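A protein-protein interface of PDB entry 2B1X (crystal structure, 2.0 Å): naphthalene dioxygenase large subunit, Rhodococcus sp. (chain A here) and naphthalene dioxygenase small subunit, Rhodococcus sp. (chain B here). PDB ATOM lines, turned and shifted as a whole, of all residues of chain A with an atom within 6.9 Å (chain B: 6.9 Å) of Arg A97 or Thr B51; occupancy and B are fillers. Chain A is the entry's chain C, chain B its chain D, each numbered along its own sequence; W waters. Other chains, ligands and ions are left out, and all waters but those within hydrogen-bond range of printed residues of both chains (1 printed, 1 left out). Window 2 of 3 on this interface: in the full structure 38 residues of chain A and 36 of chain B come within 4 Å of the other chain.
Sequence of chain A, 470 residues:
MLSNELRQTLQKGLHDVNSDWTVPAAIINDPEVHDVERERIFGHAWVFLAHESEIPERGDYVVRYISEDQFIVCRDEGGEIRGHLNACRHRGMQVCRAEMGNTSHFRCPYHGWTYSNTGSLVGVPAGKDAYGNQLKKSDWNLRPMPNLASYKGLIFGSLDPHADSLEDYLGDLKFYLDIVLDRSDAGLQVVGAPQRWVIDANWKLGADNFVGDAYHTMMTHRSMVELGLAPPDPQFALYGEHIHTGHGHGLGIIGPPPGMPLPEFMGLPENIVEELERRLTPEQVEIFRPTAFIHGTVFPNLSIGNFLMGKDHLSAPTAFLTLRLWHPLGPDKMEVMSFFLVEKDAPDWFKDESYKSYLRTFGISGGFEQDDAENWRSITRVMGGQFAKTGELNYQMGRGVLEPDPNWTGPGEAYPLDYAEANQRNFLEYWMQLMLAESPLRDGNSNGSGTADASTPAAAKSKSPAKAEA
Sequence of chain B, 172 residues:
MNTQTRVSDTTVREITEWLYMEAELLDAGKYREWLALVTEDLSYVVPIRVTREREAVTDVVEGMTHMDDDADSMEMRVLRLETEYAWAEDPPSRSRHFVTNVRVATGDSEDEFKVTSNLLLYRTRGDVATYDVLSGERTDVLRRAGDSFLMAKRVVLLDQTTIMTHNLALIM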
ATOM      1  N   TYR A  61      18.284   0.622  21.833  1.00  0.00           N
ATOM      2  CA  TYR A  61      19.408   0.137  21.040  1.00  0.00           C
ATOM      3  C   TYR A  61      19.545   0.962  19.757  1.00  0.00           C
ATOM      4  O   TYR A  61      18.572   1.521  19.273  1.00  0.00           O
ATOM      5  CB  TYR A  61      19.282  -1.347  20.685  1.00  0.00           C
ATOM      6  CG  TYR A  61      18.154  -1.634  19.729  1.00  0.00           C
ATOM      7  CD1 TYR A  61      18.330  -1.497  18.349  1.00  0.00           C
ATOM      8  CD2 TYR A  61      16.888  -2.003  20.205  1.00  0.00           C
ATOM      9  CE1 TYR A  61      17.295  -1.739  17.467  1.00  0.00           C
ATOM     10  CE2 TYR A  61      15.846  -2.250  19.340  1.00  0.00           C
ATOM     11  CZ  TYR A  61      16.057  -2.117  17.966  1.00  0.00           C
ATOM     12  OH  TYR A  61      15.026  -2.368  17.100  1.00  0.00           O
ATOM     13  N   VAL A  63      22.029   0.453  15.950  1.00  0.00           N
ATOM     14  CA  VAL A  63      22.814  -0.509  15.206  1.00  0.00           C
ATOM     15  C   VAL A  63      23.919   0.267  14.504  1.00  0.00           C
ATOM     16  O   VAL A  63      23.655   1.208  13.745  1.00  0.00           O
ATOM     17  CB  VAL A  63      21.965  -1.281  14.181  1.00  0.00           C
ATOM     18  CG1 VAL A  63      22.852  -2.180  13.363  1.00  0.00           C
ATOM     19  CG2 VAL A  63      20.904  -2.154  14.913  1.00  0.00           C
ATOM     20  N   GLN A  70      28.415  -5.453  11.819  1.00  0.00           N
ATOM     21  CA  GLN A  70      27.286  -4.737  12.366  1.00  0.00           C
ATOM     22  C   GLN A  70      27.069  -5.177  13.818  1.00  0.00           C
ATOM     23  O   GLN A  70      27.096  -6.363  14.110  1.00  0.00           O
ATOM     24  CB  GLN A  70      26.081  -5.067  11.535  1.00  0.00           C
ATOM     25  CG  GLN A  70      24.929  -4.150  11.718  1.00  0.00           C
ATOM     26  CD  GLN A  70      23.768  -4.526  10.822  1.00  0.00           C
ATOM     27  OE1 GLN A  70      23.144  -5.568  11.027  1.00  0.00           O
ATOM     28  NE2 GLN A  70      23.451  -3.656   9.847  1.00  0.00           N
ATOM     29  N   ASN A  86      25.532  -8.415  15.372  1.00  0.00           N
ATOM     30  CA  ASN A  86      24.161  -8.630  14.872  1.00  0.00           C
ATOM     31  C   ASN A  86      24.016  -9.794  13.877  1.00  0.00           C
ATOM     32  O   ASN A  86      23.608  -9.646  12.697  1.00  0.00           O
ATOM     33  CB  ASN A  86      23.627  -7.315  14.304  1.00  0.00           C
ATOM     34  CG  ASN A  86      22.129  -7.332  14.015  1.00  0.00           C
ATOM     35  OD1 ASN A  86      21.364  -8.131  14.559  1.00  0.00           O
ATOM     36  ND2 ASN A  86      21.704  -6.387  13.195  1.00  0.00           N
ATOM     37  N   MET A  93      21.784 -14.988  10.806  1.00  0.00           N
ATOM     38  CA  MET A  93      20.822 -13.948  10.413  1.00  0.00           C
ATOM     39  C   MET A  93      20.892 -12.703  11.307  1.00  0.00           C
ATOM     40  O   MET A  93      21.239 -12.808  12.485  1.00  0.00           O
ATOM     41  CB  MET A  93      19.374 -14.454  10.409  1.00  0.00           C
ATOM     42  CG  MET A  93      18.577 -13.443   9.489  1.00  0.00           C
ATOM     43  SD  MET A  93      16.975 -13.796   9.147  1.00  0.00           S
ATOM     44  CE  MET A  93      16.284 -12.086   8.914  1.00  0.00           C
ATOM     45  N   GLN A  94      20.537 -11.535  10.781  1.00  0.00           N
ATOM     46  CA  GLN A  94      20.444 -10.342  11.652  1.00  0.00           C
ATOM     47  C   GLN A  94      19.293 -10.556  12.621  1.00  0.00           C
ATOM     48  O   GLN A  94      18.157 -10.854  12.185  1.00  0.00           O
ATOM     49  CB  GLN A  94      20.140  -9.084  10.845  1.00  0.00           C
ATOM     50  CG  GLN A  94      21.271  -8.567   9.996  1.00  0.00           C
ATOM     51  CD  GLN A  94      20.759  -7.516   9.007  1.00  0.00           C
ATOM     52  OE1 GLN A  94      19.982  -7.827   8.088  1.00  0.00           O
ATOM     53  NE2 GLN A  94      21.152  -6.278   9.216  1.00  0.00           N
ATOM     54  N   VAL A  95      19.558 -10.425  13.914  1.00  0.00           N
ATOM     55  CA  VAL A  95      18.480 -10.506  14.906  1.00  0.00           C
ATOM     56  C   VAL A  95      17.786  -9.156  15.110  1.00  0.00           C
ATOM     57  O   VAL A  95      16.854  -9.036  15.872  1.00  0.00           O
ATOM     58  CB  VAL A  95      18.953 -11.123  16.247  1.00  0.00           C
ATOM     59  CG1 VAL A  95      19.406 -12.568  16.002  1.00  0.00           C
ATOM     60  CG2 VAL A  95      20.088 -10.296  16.870  1.00  0.00           C
ATOM     61  N   CYS A  96      18.265  -8.143  14.425  1.00  0.00           N
ATOM     62  CA  CYS A  96      17.656  -6.823  14.490  1.00  0.00           C
ATOM     63  C   CYS A  96      17.908  -6.191  13.134  1.00  0.00           C
ATOM     64  O   CYS A  96      19.067  -6.020  12.742  1.00  0.00           O
ATOM     65  CB  CYS A  96      18.298  -6.006  15.627  1.00  0.00           C
ATOM     66  SG  CYS A  96      17.671  -4.321  15.669  1.00  0.00           S
ATOM     67  N   ARG A  97      16.836  -5.918  12.390  1.00  0.00           N
ATOM     68  CA  ARG A  97      16.957  -5.301  11.076  1.00  0.00           C
ATOM     69  C   ARG A  97      16.492  -3.829  11.050  1.00  0.00           C
ATOM     70  O   ARG A  97      16.444  -3.225   9.963  1.00  0.00           O
ATOM     71  CB  ARG A  97      16.240  -6.120   9.982  1.00  0.00           C
ATOM     72  CG  ARG A  97      16.980  -7.348   9.477  1.00  0.00           C
ATOM     73  CD  ARG A  97      16.083  -8.368   8.695  1.00  0.00           C
ATOM     74  NE  ARG A  97      14.875  -8.655   9.483  1.00  0.00           N
ATOM     75  CZ  ARG A  97      13.637  -8.623   9.039  1.00  0.00           C
ATOM     76  NH1 ARG A  97      13.375  -8.367   7.754  1.00  0.00           N
ATOM     77  NH2 ARG A  97      12.644  -8.844   9.897  1.00  0.00           N
ATOM     78  N   ALA A  98      16.167  -3.279  12.225  1.00  0.00           N
ATOM     79  CA  ALA A  98      15.896  -1.835  12.397  1.00  0.00           C
ATOM     80  C   ALA A  98      17.225  -1.093  12.673  1.00  0.00           C
ATOM     81  O   ALA A  98      18.206  -1.724  13.073  1.00  0.00           O
ATOM     82  CB  ALA A  98      14.923  -1.610  13.562  1.00  0.00           C
ATOM     83  N   GLU A  99      17.243   0.228  12.503  1.00  0.00           N
ATOM     84  CA  GLU A  99      18.456   1.049  12.788  1.00  0.00           C
ATOM     85  C   GLU A  99      18.558   1.465  14.255  1.00  0.00           C
ATOM     86  O   GLU A  99      19.656   1.786  14.758  1.00  0.00           O
ATOM     87  CB  GLU A  99      18.490   2.283  11.883  1.00  0.00           C
ATOM     88  CG  GLU A  99      18.505   1.884  10.402  1.00  0.00           C
ATOM     89  CD  GLU A  99      18.447   3.055   9.444  1.00  0.00           C
ATOM     90  OE1 GLU A  99      18.969   4.142   9.796  1.00  0.00           O
ATOM     91  OE2 GLU A  99      17.948   2.881   8.317  1.00  0.00           O
ATOM     92  N   MET A 100      17.418   1.435  14.932  1.00  0.00           N
ATOM     93  CA  MET A 100      17.316   1.781  16.349  1.00  0.00           C
ATOM     94  C   MET A 100      15.914   1.401  16.824  1.00  0.00           C
ATOM     95  O   MET A 100      15.051   1.130  16.001  1.00  0.00           O
ATOM     96  CB  MET A 100      17.536   3.290  16.569  1.00  0.00           C
ATOM     97  CG  MET A 100      16.645   4.181  15.749  1.00  0.00           C
ATOM     98  SD  MET A 100      17.077   5.928  15.955  1.00  0.00           S
ATOM     99  CE  MET A 100      15.526   6.560  15.973  1.00  0.00           C
ATOM    100  N   GLY A 101      15.697   1.405  18.134  1.00  0.00           N
ATOM    101  CA  GLY A 101      14.425   0.996  18.722  1.00  0.00           C
ATOM    102  C   GLY A 101      14.562   0.677  20.192  1.00  0.00           C
ATOM    103  O   GLY A 101      15.540   1.037  20.823  1.00  0.00           O
ATOM    104  N   PRO A 109      14.385 -14.126  12.977  1.00  0.00           N
ATOM    105  CA  PRO A 109      13.278 -14.516  12.088  1.00  0.00           C
ATOM    106  C   PRO A 109      13.461 -15.867  11.384  1.00  0.00           C
ATOM    107  O   PRO A 109      12.478 -16.475  10.910  1.00  0.00           O
ATOM    108  CB  PRO A 109      13.252 -13.381  11.050  1.00  0.00           C
ATOM    109  CG  PRO A 109      13.864 -12.262  11.744  1.00  0.00           C
ATOM    110  CD  PRO A 109      15.032 -12.880  12.503  1.00  0.00           C
ATOM    111  N   ARG B  49      14.947   9.873   8.163  1.00  0.00           N
ATOM    112  CA  ARG B  49      14.218   8.648   8.427  1.00  0.00           C
ATOM    113  C   ARG B  49      15.155   7.563   8.876  1.00  0.00           C
ATOM    114  O   ARG B  49      16.329   7.541   8.459  1.00  0.00           O
ATOM    115  CB  ARG B  49      13.468   8.194   7.157  1.00  0.00           C
ATOM    116  CG  ARG B  49      12.346   9.172   6.763  1.00  0.00           C
ATOM    117  CD  ARG B  49      11.566   8.755   5.566  1.00  0.00           C
ATOM    118  NE  ARG B  49      10.714   7.606   5.888  1.00  0.00           N
ATOM    119  CZ  ARG B  49      10.028   6.945   4.994  1.00  0.00           C
ATOM    120  NH1 ARG B  49      10.075   7.328   3.720  1.00  0.00           N
ATOM    121  NH2 ARG B  49       9.309   5.898   5.362  1.00  0.00           N
ATOM    122  N   VAL B  50      14.657   6.672   9.726  1.00  0.00           N
ATOM    123  CA  VAL B  50      15.403   5.484  10.118  1.00  0.00           C
ATOM    124  C   VAL B  50      14.545   4.247   9.888  1.00  0.00           C
ATOM    125  O   VAL B  50      13.315   4.295  10.014  1.00  0.00           O
ATOM    126  CB  VAL B  50      15.895   5.532  11.624  1.00  0.00           C
ATOM    127  CG1 VAL B  50      17.007   6.614  11.810  1.00  0.00           C
ATOM    128  CG2 VAL B  50      14.726   5.754  12.601  1.00  0.00           C
ATOM    129  N   THR B  51      15.183   3.132   9.570  1.00  0.00           N
ATOM    130  CA  THR B  51      14.463   1.892   9.419  1.00  0.00           C
ATOM    131  C   THR B  51      13.896   1.458  10.770  1.00  0.00           C
ATOM    132  O   THR B  51      14.655   1.352  11.752  1.00  0.00           O
ATOM    133  CB  THR B  51      15.415   0.778   8.931  1.00  0.00           C
ATOM    134  OG1 THR B  51      16.044   1.195   7.712  1.00  0.00           O
ATOM    135  CG2 THR B  51      14.603  -0.481   8.565  1.00  0.00           C
ATOM    136  N   ARG B  52      12.603   1.153  10.788  1.00  0.00           N
ATOM    137  CA  ARG B  52      11.934   0.666  11.994  1.00  0.00           C
ATOM    138  C   ARG B  52      10.976  -0.454  11.653  1.00  0.00           C
ATOM    139  O   ARG B  52      10.522  -0.556  10.526  1.00  0.00           O
ATOM    140  CB  ARG B  52      11.217   1.803  12.725  1.00  0.00           C
ATOM    141  CG  ARG B  52      12.170   2.916  13.074  1.00  0.00           C
ATOM    142  CD  ARG B  52      11.847   3.755  14.249  1.00  0.00           C
ATOM    143  NE  ARG B  52      11.486   2.981  15.433  1.00  0.00           N
ATOM    144  CZ  ARG B  52      10.574   3.409  16.290  1.00  0.00           C
ATOM    145  NH1 ARG B  52       9.984   4.590  16.061  1.00  0.00           N
ATOM    146  NH2 ARG B  52      10.252   2.683  17.357  1.00  0.00           N
ATOM    147  N   GLU B  53      10.666  -1.284  12.637  1.00  0.00           N
ATOM    148  CA  GLU B  53       9.603  -2.277  12.493  1.00  0.00           C
ATOM    149  C   GLU B  53       8.280  -1.590  12.142  1.00  0.00           C
ATOM    150  O   GLU B  53       8.074  -0.404  12.451  1.00  0.00           O
ATOM    151  CB  GLU B  53       9.487  -3.159  13.762  1.00  0.00           C
ATOM    152  CG  GLU B  53       9.077  -2.409  15.025  1.00  0.00           C
ATOM    153  CD  GLU B  53      10.270  -1.992  15.877  1.00  0.00           C
ATOM    154  OE1 GLU B  53      11.331  -1.644  15.285  1.00  0.00           O
ATOM    155  OE2 GLU B  53      10.147  -2.012  17.147  1.00  0.00           O
ATOM    156  N   ASP B  59       8.722   6.624  11.541  1.00  0.00           N
ATOM    157  CA  ASP B  59      10.135   6.376  11.327  1.00  0.00           C
ATOM    158  C   ASP B  59      10.858   7.696  11.008  1.00  0.00           C
ATOM    159  O   ASP B  59      12.025   7.676  10.658  1.00  0.00           O
ATOM    160  CB  ASP B  59      10.362   5.298  10.249  1.00  0.00           C
ATOM    161  CG  ASP B  59       9.824   5.691   8.865  1.00  0.00           C
ATOM    162  OD1 ASP B  59       9.567   6.887   8.615  1.00  0.00           O
ATOM    163  OD2 ASP B  59       9.672   4.852   7.941  1.00  0.00           O
ATOM    164  N   THR B 161      16.883   6.126   3.990  1.00  0.00           N
ATOM    165  CA  THR B 161      17.356   6.496   5.321  1.00  0.00           C
ATOM    166  C   THR B 161      18.770   7.107   5.143  1.00  0.00           C
ATOM    167  O   THR B 161      18.961   8.320   5.227  1.00  0.00           O
ATOM    168  CB  THR B 161      17.272   5.299   6.321  1.00  0.00           C
ATOM    169  OG1 THR B 161      17.838   4.116   5.740  1.00  0.00           O
ATOM    170  CG2 THR B 161      15.805   4.874   6.525  1.00  0.00           C
HETATM  171  O   HOH W   1      12.440  -2.615  18.084  1.00  0.00           O
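Water W1 lies within hydrogen-bond range of OE2 of Glu B53 (2.5 Å) and OH of Tyr A61 (2.8 Å).
O of Glu A99 lies within hydrogen-bond range of N of Val A63, 3.0 Å away.
O of Ala A98 lies within hydrogen-bond range of SG of Cys A96.
The backbone carbonyl oxygen of Asp B59 lies within hydrogen-bond range of the backbone NH of Val B50 (3.0 Å).
Hydrophobic or aromatic side chains of chain A that line the printed part of chain B: Ala A98 and Met A100.
Among the printed residues, 7 pairs touch across the chains.
Among the printed residues, no Asp or Glu carboxylate lies within 4 Å of a Lys or Arg side-chain nitrogen of the other chain.
Cys A96 touches none of the printed residues of chain B.
Of the printed residues of chain B, Arg A97 touches Thr B51 (3.6 Å).
Printed residues of chain B within 4 Å of Ala A98: Thr B51 and Glu B53.
Of the printed residues of chain B, Glu A99 touches Val B50, Thr B51 and Thr B161.
Printed residues of chain A within 4 Å of Val B50: Glu A99 (3.7 Å) and Met A100 (3.6 Å).
Arg B52 touches none of the printed residues of chain A.
Of the printed residues of chain A, Glu B53 touches Ala A98.
The nearest residue of chain B that does not touch Arg A97 is Arg B52 (5.9 Å).
The nearest residue of chain A that does not touch Thr B51 is Met A100 (4.2 Å).
The nearest printed residue of chain A that does not touch Thr B161 is Arg A97 (8.6 Å).
Among the printed residues, merely in contact across the chains: Ala A98 with Thr B51 (3.5 Å), Met A100 with Val B50 (3.6 Å), Arg A97 with Thr B51 (3.6 Å), Glu A99 with Val B50 (3.7 Å) and Ala A98 with Glu B53 (3.98 Å).
The side-chain carboxylate of Glu A99 lies within hydrogen-bond range of the side-chain hydroxyl of Thr B161 (2.9 Å).
The side-chain carboxylate (OE2) of Glu A99 lies within hydrogen-bond range of the side-chain hydroxyl (OG1) of Thr B51, at 2.6 Å.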
